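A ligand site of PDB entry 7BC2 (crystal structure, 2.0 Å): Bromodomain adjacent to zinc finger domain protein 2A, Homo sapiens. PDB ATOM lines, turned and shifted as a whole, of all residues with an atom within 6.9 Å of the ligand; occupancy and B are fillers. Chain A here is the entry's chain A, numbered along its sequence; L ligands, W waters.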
ATOM      1  N   TRP A  23       6.167 -14.224  14.939  1.00  0.00           N
ATOM      2  CA  TRP A  23       7.041 -13.248  14.289  1.00  0.00           C
ATOM      3  C   TRP A  23       8.125 -13.843  13.392  1.00  0.00           C
ATOM      4  O   TRP A  23       8.435 -13.212  12.372  1.00  0.00           O
ATOM      5  CB  TRP A  23       7.657 -12.319  15.356  1.00  0.00           C
ATOM      6  CG  TRP A  23       8.538 -13.002  16.339  1.00  0.00           C
ATOM      7  CD1 TRP A  23       8.189 -13.477  17.572  1.00  0.00           C
ATOM      8  CD2 TRP A  23       9.939 -13.285  16.176  1.00  0.00           C
ATOM      9  NE1 TRP A  23       9.284 -14.048  18.182  1.00  0.00           N
ATOM     10  CE2 TRP A  23      10.367 -13.934  17.346  1.00  0.00           C
ATOM     11  CE3 TRP A  23      10.870 -13.053  15.157  1.00  0.00           C
ATOM     12  CZ2 TRP A  23      11.688 -14.364  17.531  1.00  0.00           C
ATOM     13  CZ3 TRP A  23      12.177 -13.473  15.343  1.00  0.00           C
ATOM     14  CH2 TRP A  23      12.568 -14.114  16.511  1.00  0.00           C
ATOM     15  N   PRO A  24       8.710 -15.028  13.650  1.00  0.00           N
ATOM     16  CA  PRO A  24       9.717 -15.525  12.686  1.00  0.00           C
ATOM     17  C   PRO A  24       9.122 -16.010  11.376  1.00  0.00           C
ATOM     18  O   PRO A  24       9.888 -16.245  10.442  1.00  0.00           O
ATOM     19  CB  PRO A  24      10.385 -16.692  13.418  1.00  0.00           C
ATOM     20  CG  PRO A  24       9.934 -16.583  14.870  1.00  0.00           C
ATOM     21  CD  PRO A  24       8.578 -15.945  14.792  1.00  0.00           C
ATOM     22  N   PHE A  25       7.801 -16.202  11.295  1.00  0.00           N
ATOM     23  CA  PHE A  25       7.209 -16.950  10.190  1.00  0.00           C
ATOM     24  C   PHE A  25       6.215 -16.133   9.389  1.00  0.00           C
ATOM     25  O   PHE A  25       5.522 -16.686   8.529  1.00  0.00           O
ATOM     26  CB  PHE A  25       6.529 -18.218  10.724  1.00  0.00           C
ATOM     27  CG  PHE A  25       7.340 -18.914  11.767  1.00  0.00           C
ATOM     28  CD1 PHE A  25       8.499 -19.583  11.423  1.00  0.00           C
ATOM     29  CD2 PHE A  25       6.953 -18.871  13.102  1.00  0.00           C
ATOM     30  CE1 PHE A  25       9.274 -20.219  12.378  1.00  0.00           C
ATOM     31  CE2 PHE A  25       7.722 -19.517  14.066  1.00  0.00           C
ATOM     32  CZ  PHE A  25       8.880 -20.186  13.708  1.00  0.00           C
ATOM     33  N   LEU A  26       6.103 -14.829   9.664  1.00  0.00           N
ATOM     34  CA  LEU A  26       5.126 -13.982   8.989  1.00  0.00           C
ATOM     35  C   LEU A  26       5.508 -13.694   7.549  1.00  0.00           C
ATOM     36  O   LEU A  26       4.615 -13.444   6.730  1.00  0.00           O
ATOM     37  CB  LEU A  26       4.976 -12.665   9.748  1.00  0.00           C
ATOM     38  CG  LEU A  26       4.429 -12.788  11.170  1.00  0.00           C
ATOM     39  CD1 LEU A  26       4.427 -11.415  11.829  1.00  0.00           C
ATOM     40  CD2 LEU A  26       3.031 -13.373  11.105  1.00  0.00           C
ATOM     41  N   GLU A  27       6.805 -13.679   7.233  1.00  0.00           N
ATOM     42  CA  GLU A  27       7.341 -13.357   5.921  1.00  0.00           C
ATOM     43  C   GLU A  27       8.396 -14.389   5.561  1.00  0.00           C
ATOM     44  O   GLU A  27       8.982 -15.010   6.451  1.00  0.00           O
ATOM     45  CB  GLU A  27       7.983 -11.955   5.901  1.00  0.00           C
ATOM     46  CG  GLU A  27       7.028 -10.808   6.189  1.00  0.00           C
ATOM     47  CD  GLU A  27       6.011 -10.609   5.088  1.00  0.00           C
ATOM     48  OE1 GLU A  27       6.354 -10.835   3.900  1.00  0.00           O
ATOM     49  OE2 GLU A  27       4.863 -10.219   5.393  1.00  0.00           O
ATOM     50  N   PRO A  28       8.666 -14.597   4.270  1.00  0.00           N
ATOM     51  CA  PRO A  28       9.782 -15.467   3.874  1.00  0.00           C
ATOM     52  C   PRO A  28      11.071 -15.062   4.576  1.00  0.00           C
ATOM     53  O   PRO A  28      11.369 -13.874   4.740  1.00  0.00           O
ATOM     54  CB  PRO A  28       9.893 -15.256   2.366  1.00  0.00           C
ATOM     55  CG  PRO A  28       8.539 -14.826   1.958  1.00  0.00           C
ATOM     56  CD  PRO A  28       7.991 -14.015   3.100  1.00  0.00           C
ATOM     57  N   VAL A  29      11.841 -16.063   5.015  1.00  0.00           N
ATOM     58  CA  VAL A  29      13.163 -15.775   5.525  1.00  0.00           C
ATOM     59  C   VAL A  29      13.996 -15.176   4.408  1.00  0.00           C
ATOM     60  O   VAL A  29      13.992 -15.684   3.276  1.00  0.00           O
ATOM     61  CB  VAL A  29      13.826 -17.050   6.050  1.00  0.00           C
ATOM     62  CG1 VAL A  29      15.299 -16.786   6.359  1.00  0.00           C
ATOM     63  CG2 VAL A  29      13.091 -17.568   7.268  1.00  0.00           C
ATOM     64  N   ASN A  30      14.687 -14.076   4.700  1.00  0.00           N
ATOM     65  CA  ASN A  30      15.512 -13.408   3.691  1.00  0.00           C
ATOM     66  C   ASN A  30      16.896 -14.044   3.715  1.00  0.00           C
ATOM     67  O   ASN A  30      17.660 -13.799   4.656  1.00  0.00           O
ATOM     68  CB  ASN A  30      15.588 -11.918   3.976  1.00  0.00           C
ATOM     69  CG  ASN A  30      16.326 -11.161   2.880  1.00  0.00           C
ATOM     70  OD1 ASN A  30      17.134 -11.728   2.152  1.00  0.00           O
ATOM     71  ND2 ASN A  30      16.038  -9.869   2.773  1.00  0.00           N
ATOM     72  N   PRO A  31      17.283 -14.831   2.704  1.00  0.00           N
ATOM     73  CA  PRO A  31      18.557 -15.541   2.793  1.00  0.00           C
ATOM     74  C   PRO A  31      19.758 -14.612   2.811  1.00  0.00           C
ATOM     75  O   PRO A  31      20.820 -15.013   3.290  1.00  0.00           O
ATOM     76  CB  PRO A  31      18.550 -16.438   1.546  1.00  0.00           C
ATOM     77  CG  PRO A  31      17.692 -15.705   0.581  1.00  0.00           C
ATOM     78  CD  PRO A  31      16.609 -15.038   1.407  1.00  0.00           C
ATOM     79  N   LEU A  33      20.099 -12.260   4.734  1.00  0.00           N
ATOM     80  CA  LEU A  33      20.254 -11.870   6.136  1.00  0.00           C
ATOM     81  C   LEU A  33      20.492 -13.053   7.058  1.00  0.00           C
ATOM     82  O   LEU A  33      20.839 -12.845   8.224  1.00  0.00           O
ATOM     83  CB  LEU A  33      18.993 -11.116   6.595  1.00  0.00           C
ATOM     84  CG  LEU A  33      18.620  -9.878   5.785  1.00  0.00           C
ATOM     85  CD1 LEU A  33      17.295  -9.306   6.252  1.00  0.00           C
ATOM     86  CD2 LEU A  33      19.711  -8.844   5.912  1.00  0.00           C
ATOM     87  N   VAL A  34      20.293 -14.285   6.579  1.00  0.00           N
ATOM     88  CA  VAL A  34      20.401 -15.491   7.392  1.00  0.00           C
ATOM     89  C   VAL A  34      21.382 -16.413   6.694  1.00  0.00           C
ATOM     90  O   VAL A  34      21.022 -17.134   5.763  1.00  0.00           O
ATOM     91  CB  VAL A  34      19.045 -16.178   7.592  1.00  0.00           C
ATOM     92  CG1 VAL A  34      19.212 -17.433   8.446  1.00  0.00           C
ATOM     93  CG2 VAL A  34      18.057 -15.216   8.248  1.00  0.00           C
ATOM     94  N   TYR A  37      20.865 -20.314   5.122  1.00  0.00           N
ATOM     95  CA  TYR A  37      19.468 -20.729   5.051  1.00  0.00           C
ATOM     96  C   TYR A  37      19.121 -21.336   3.697  1.00  0.00           C
ATOM     97  O   TYR A  37      18.409 -22.349   3.630  1.00  0.00           O
ATOM     98  CB  TYR A  37      18.542 -19.542   5.350  1.00  0.00           C
ATOM     99  CG  TYR A  37      17.128 -19.981   5.652  1.00  0.00           C
ATOM    100  CD1 TYR A  37      16.790 -20.416   6.921  1.00  0.00           C
ATOM    101  CD2 TYR A  37      16.154 -20.012   4.650  1.00  0.00           C
ATOM    102  CE1 TYR A  37      15.504 -20.851   7.219  1.00  0.00           C
ATOM    103  CE2 TYR A  37      14.860 -20.447   4.943  1.00  0.00           C
ATOM    104  CZ  TYR A  37      14.552 -20.861   6.221  1.00  0.00           C
ATOM    105  OH  TYR A  37      13.280 -21.286   6.517  1.00  0.00           O
ATOM    106  N   ILE A  41      17.690 -25.174   3.631  1.00  0.00           N
ATOM    107  CA  ILE A  41      16.237 -25.300   3.541  1.00  0.00           C
ATOM    108  C   ILE A  41      15.862 -25.406   2.058  1.00  0.00           C
ATOM    109  O   ILE A  41      15.991 -24.443   1.302  1.00  0.00           O
ATOM    110  CB  ILE A  41      15.508 -24.130   4.211  1.00  0.00           C
ATOM    111  CG1 ILE A  41      15.723 -24.190   5.730  1.00  0.00           C
ATOM    112  CG2 ILE A  41      14.010 -24.155   3.878  1.00  0.00           C
ATOM    113  CD1 ILE A  41      15.313 -25.551   6.374  1.00  0.00           C
ATOM    114  N   VAL A  72       6.316 -25.263   7.360  1.00  0.00           N
ATOM    115  CA  VAL A  72       6.873 -24.122   8.115  1.00  0.00           C
ATOM    116  C   VAL A  72       7.626 -24.632   9.346  1.00  0.00           C
ATOM    117  O   VAL A  72       8.754 -24.218   9.628  1.00  0.00           O
ATOM    118  CB  VAL A  72       5.753 -23.132   8.512  1.00  0.00           C
ATOM    119  CG1 VAL A  72       6.316 -22.043   9.395  1.00  0.00           C
ATOM    120  CG2 VAL A  72       5.094 -22.500   7.269  1.00  0.00           C
ATOM    121  N   ASN A  75      10.797 -26.922   8.586  1.00  0.00           N
ATOM    122  CA  ASN A  75      11.940 -26.081   8.232  1.00  0.00           C
ATOM    123  C   ASN A  75      12.516 -25.395   9.460  1.00  0.00           C
ATOM    124  O   ASN A  75      13.738 -25.317   9.626  1.00  0.00           O
ATOM    125  CB  ASN A  75      11.526 -25.002   7.213  1.00  0.00           C
ATOM    126  CG  ASN A  75      11.226 -25.567   5.845  1.00  0.00           C
ATOM    127  OD1 ASN A  75      11.644 -26.681   5.506  1.00  0.00           O
ATOM    128  ND2 ASN A  75      10.531 -24.790   5.029  1.00  0.00           N
ATOM    129  N   CYS A  76      11.631 -24.883  10.328  1.00  0.00           N
ATOM    130  CA  CYS A  76      12.103 -24.210  11.528  1.00  0.00           C
ATOM    131  C   CYS A  76      12.977 -25.132  12.360  1.00  0.00           C
ATOM    132  O   CYS A  76      14.060 -24.731  12.820  1.00  0.00           O
ATOM    133  CB  CYS A  76      10.910 -23.717  12.340  1.00  0.00           C
ATOM    134  SG  CYS A  76      11.406 -22.938  13.874  1.00  0.00           S
ATOM    135  N   PHE A  79      16.453 -25.801  10.637  1.00  0.00           N
ATOM    136  CA  PHE A  79      17.446 -24.738  10.628  1.00  0.00           C
ATOM    137  C   PHE A  79      17.816 -24.241  12.021  1.00  0.00           C
ATOM    138  O   PHE A  79      18.982 -23.885  12.254  1.00  0.00           O
ATOM    139  CB  PHE A  79      16.969 -23.543   9.790  1.00  0.00           C
ATOM    140  CG  PHE A  79      18.030 -22.506   9.607  1.00  0.00           C
ATOM    141  CD1 PHE A  79      19.034 -22.684   8.653  1.00  0.00           C
ATOM    142  CD2 PHE A  79      18.066 -21.374  10.424  1.00  0.00           C
ATOM    143  CE1 PHE A  79      20.038 -21.739   8.499  1.00  0.00           C
ATOM    144  CE2 PHE A  79      19.070 -20.419  10.270  1.00  0.00           C
ATOM    145  CZ  PHE A  79      20.061 -20.606   9.317  1.00  0.00           C
ATOM    146  N   ASN A  80      16.873 -24.222  12.965  1.00  0.00           N
ATOM    147  CA  ASN A  80      17.072 -23.559  14.248  1.00  0.00           C
ATOM    148  C   ASN A  80      17.163 -24.579  15.379  1.00  0.00           C
ATOM    149  O   ASN A  80      16.421 -25.574  15.402  1.00  0.00           O
ATOM    150  CB  ASN A  80      15.944 -22.578  14.540  1.00  0.00           C
ATOM    151  CG  ASN A  80      15.756 -21.581  13.423  1.00  0.00           C
ATOM    152  OD1 ASN A  80      16.392 -20.530  13.423  1.00  0.00           O
ATOM    153  ND2 ASN A  80      14.912 -21.918  12.457  1.00  0.00           N
ATOM    154  N   VAL A  86      14.216 -18.437  17.789  1.00  0.00           N
ATOM    155  CA  VAL A  86      13.307 -18.805  16.711  1.00  0.00           C
ATOM    156  C   VAL A  86      12.785 -20.215  16.921  1.00  0.00           C
ATOM    157  O   VAL A  86      11.601 -20.491  16.726  1.00  0.00           O
ATOM    158  CB  VAL A  86      14.006 -18.647  15.353  1.00  0.00           C
ATOM    159  CG1 VAL A  86      13.174 -19.283  14.248  1.00  0.00           C
ATOM    160  CG2 VAL A  86      14.245 -17.155  15.034  1.00  0.00           C
HETATM  161  C1  LIG L   1      14.834 -12.723  12.197  1.00  0.00           C
HETATM  162  C2  LIG L   1      14.045 -11.527  12.162  1.00  0.00           C
HETATM  163  C3  LIG L   1      14.639 -10.192  12.627  1.00  0.00           C
HETATM  164  N1  LIG L   1      15.275  -9.552  11.788  1.00  0.00           N
HETATM  165  C4  LIG L   1      16.525  -9.612  11.821  1.00  0.00           C
HETATM  166  C5  LIG L   1      16.951  -8.685  10.636  1.00  0.00           C
HETATM  167  C6  LIG L   1      15.780  -8.602   9.727  1.00  0.00           C
HETATM  168  C7  LIG L   1      14.838  -9.389  10.245  1.00  0.00           C
HETATM  169  C8  LIG L   1      14.740 -10.551   9.195  1.00  0.00           C
HETATM  170  C9  LIG L   1      15.605 -11.614   9.191  1.00  0.00           C
HETATM  171  C10 LIG L   1      15.458 -12.629   8.234  1.00  0.00           C
HETATM  172  N2  LIG L   1      14.485 -12.570   7.311  1.00  0.00           N
HETATM  173  C11 LIG L   1      13.639 -11.577   7.276  1.00  0.00           C
HETATM  174  C12 LIG L   1      13.731 -10.533   8.205  1.00  0.00           C
HETATM  175  C13 LIG L   1      12.715 -11.585  11.704  1.00  0.00           C
HETATM  176  C14 LIG L   1      12.155 -12.799  11.256  1.00  0.00           C
HETATM  177  C15 LIG L   1      16.322 -17.886  11.141  1.00  0.00           C
HETATM  178  C16 LIG L   1      12.740 -18.156  10.581  1.00  0.00           C
HETATM  179  C17 LIG L   1      13.847 -17.413  10.896  1.00  0.00           C
HETATM  180  C18 LIG L   1      13.800 -16.026  11.147  1.00  0.00           C
HETATM  181  C19 LIG L   1      14.253 -13.967  11.745  1.00  0.00           C
HETATM  182  C20 LIG L   1      12.965 -14.004  11.281  1.00  0.00           C
HETATM  183  N3  LIG L   1      14.908 -18.229  10.873  1.00  0.00           N
HETATM  184  N4  LIG L   1      14.456 -19.481  10.566  1.00  0.00           N
HETATM  185  N5  LIG L   1      13.113 -19.422  10.390  1.00  0.00           N
HETATM  186  N6  LIG L   1      14.749 -15.251  11.658  1.00  0.00           N
HETATM  187  N7  LIG L   1      12.700 -15.299  10.926  1.00  0.00           N
HETATM  188  O   HOH W   1      11.000 -13.994   8.230  1.00  0.00           O
HETATM  189  O   HOH W   2      17.412 -15.298  12.907  1.00  0.00           O
HETATM  190  O   HOH W   3      12.716 -21.822   9.061  1.00  0.00           O
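The backbone NH (N) of Asn 30 sits at hydrogen-bond distance from a nitrogen (N2) of the ligand (3.0 Å). The backbone carbonyl oxygen of Pro 24 lies close to a nitrogen (N7) of the ligand, at 3.0 Å. The side-chain amide nitrogen (ND2) of Asn 80 sits at hydrogen-bond distance from a nitrogen (N4) of the ligand (3.1 Å).
The backbone carbonyl oxygen of Val 86 sits at hydrogen-bond distance from the side-chain sulfur of Cys 76. O of Cys 76 lies within hydrogen-bond range of ND2 of Asn 80 (3.0 Å).
O of Trp 23 touches C14 of the ligand (3.9 Å). Val 29 touches the ligand (CG2 to C16, 3.4 Å). Leu 33 touches the ligand (CD1 to C6, 3.9 Å). Val 34 touches the ligand (CG2 to C10, 3.7 Å). Tyr 37 touches the ligand (CE1 to N4, 3.8 Å). Phe 79 touches the ligand. Val 86 touches the ligand (CG1 to C16, 3.9 Å). Hydrophobic or aromatic side chains that line the ligand: Pro 24, Val 29, Leu 33, Val 34, Tyr 37, Phe 79 and Val 86.
Water W3 lies within hydrogen-bond range of the side-chain hydroxyl of Tyr 37 (2.7 Å), a nitrogen (N5) of the ligand (2.8 Å) and the backbone NH of Cys 76 (3.5 Å). Water W1 lies within hydrogen-bond range of the backbone carbonyl oxygen of Glu 27 (2.9 Å), the backbone carbonyl oxygen of Pro 24 (3.3 Å) and a nitrogen (N7) of the ligand (3.4 Å).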
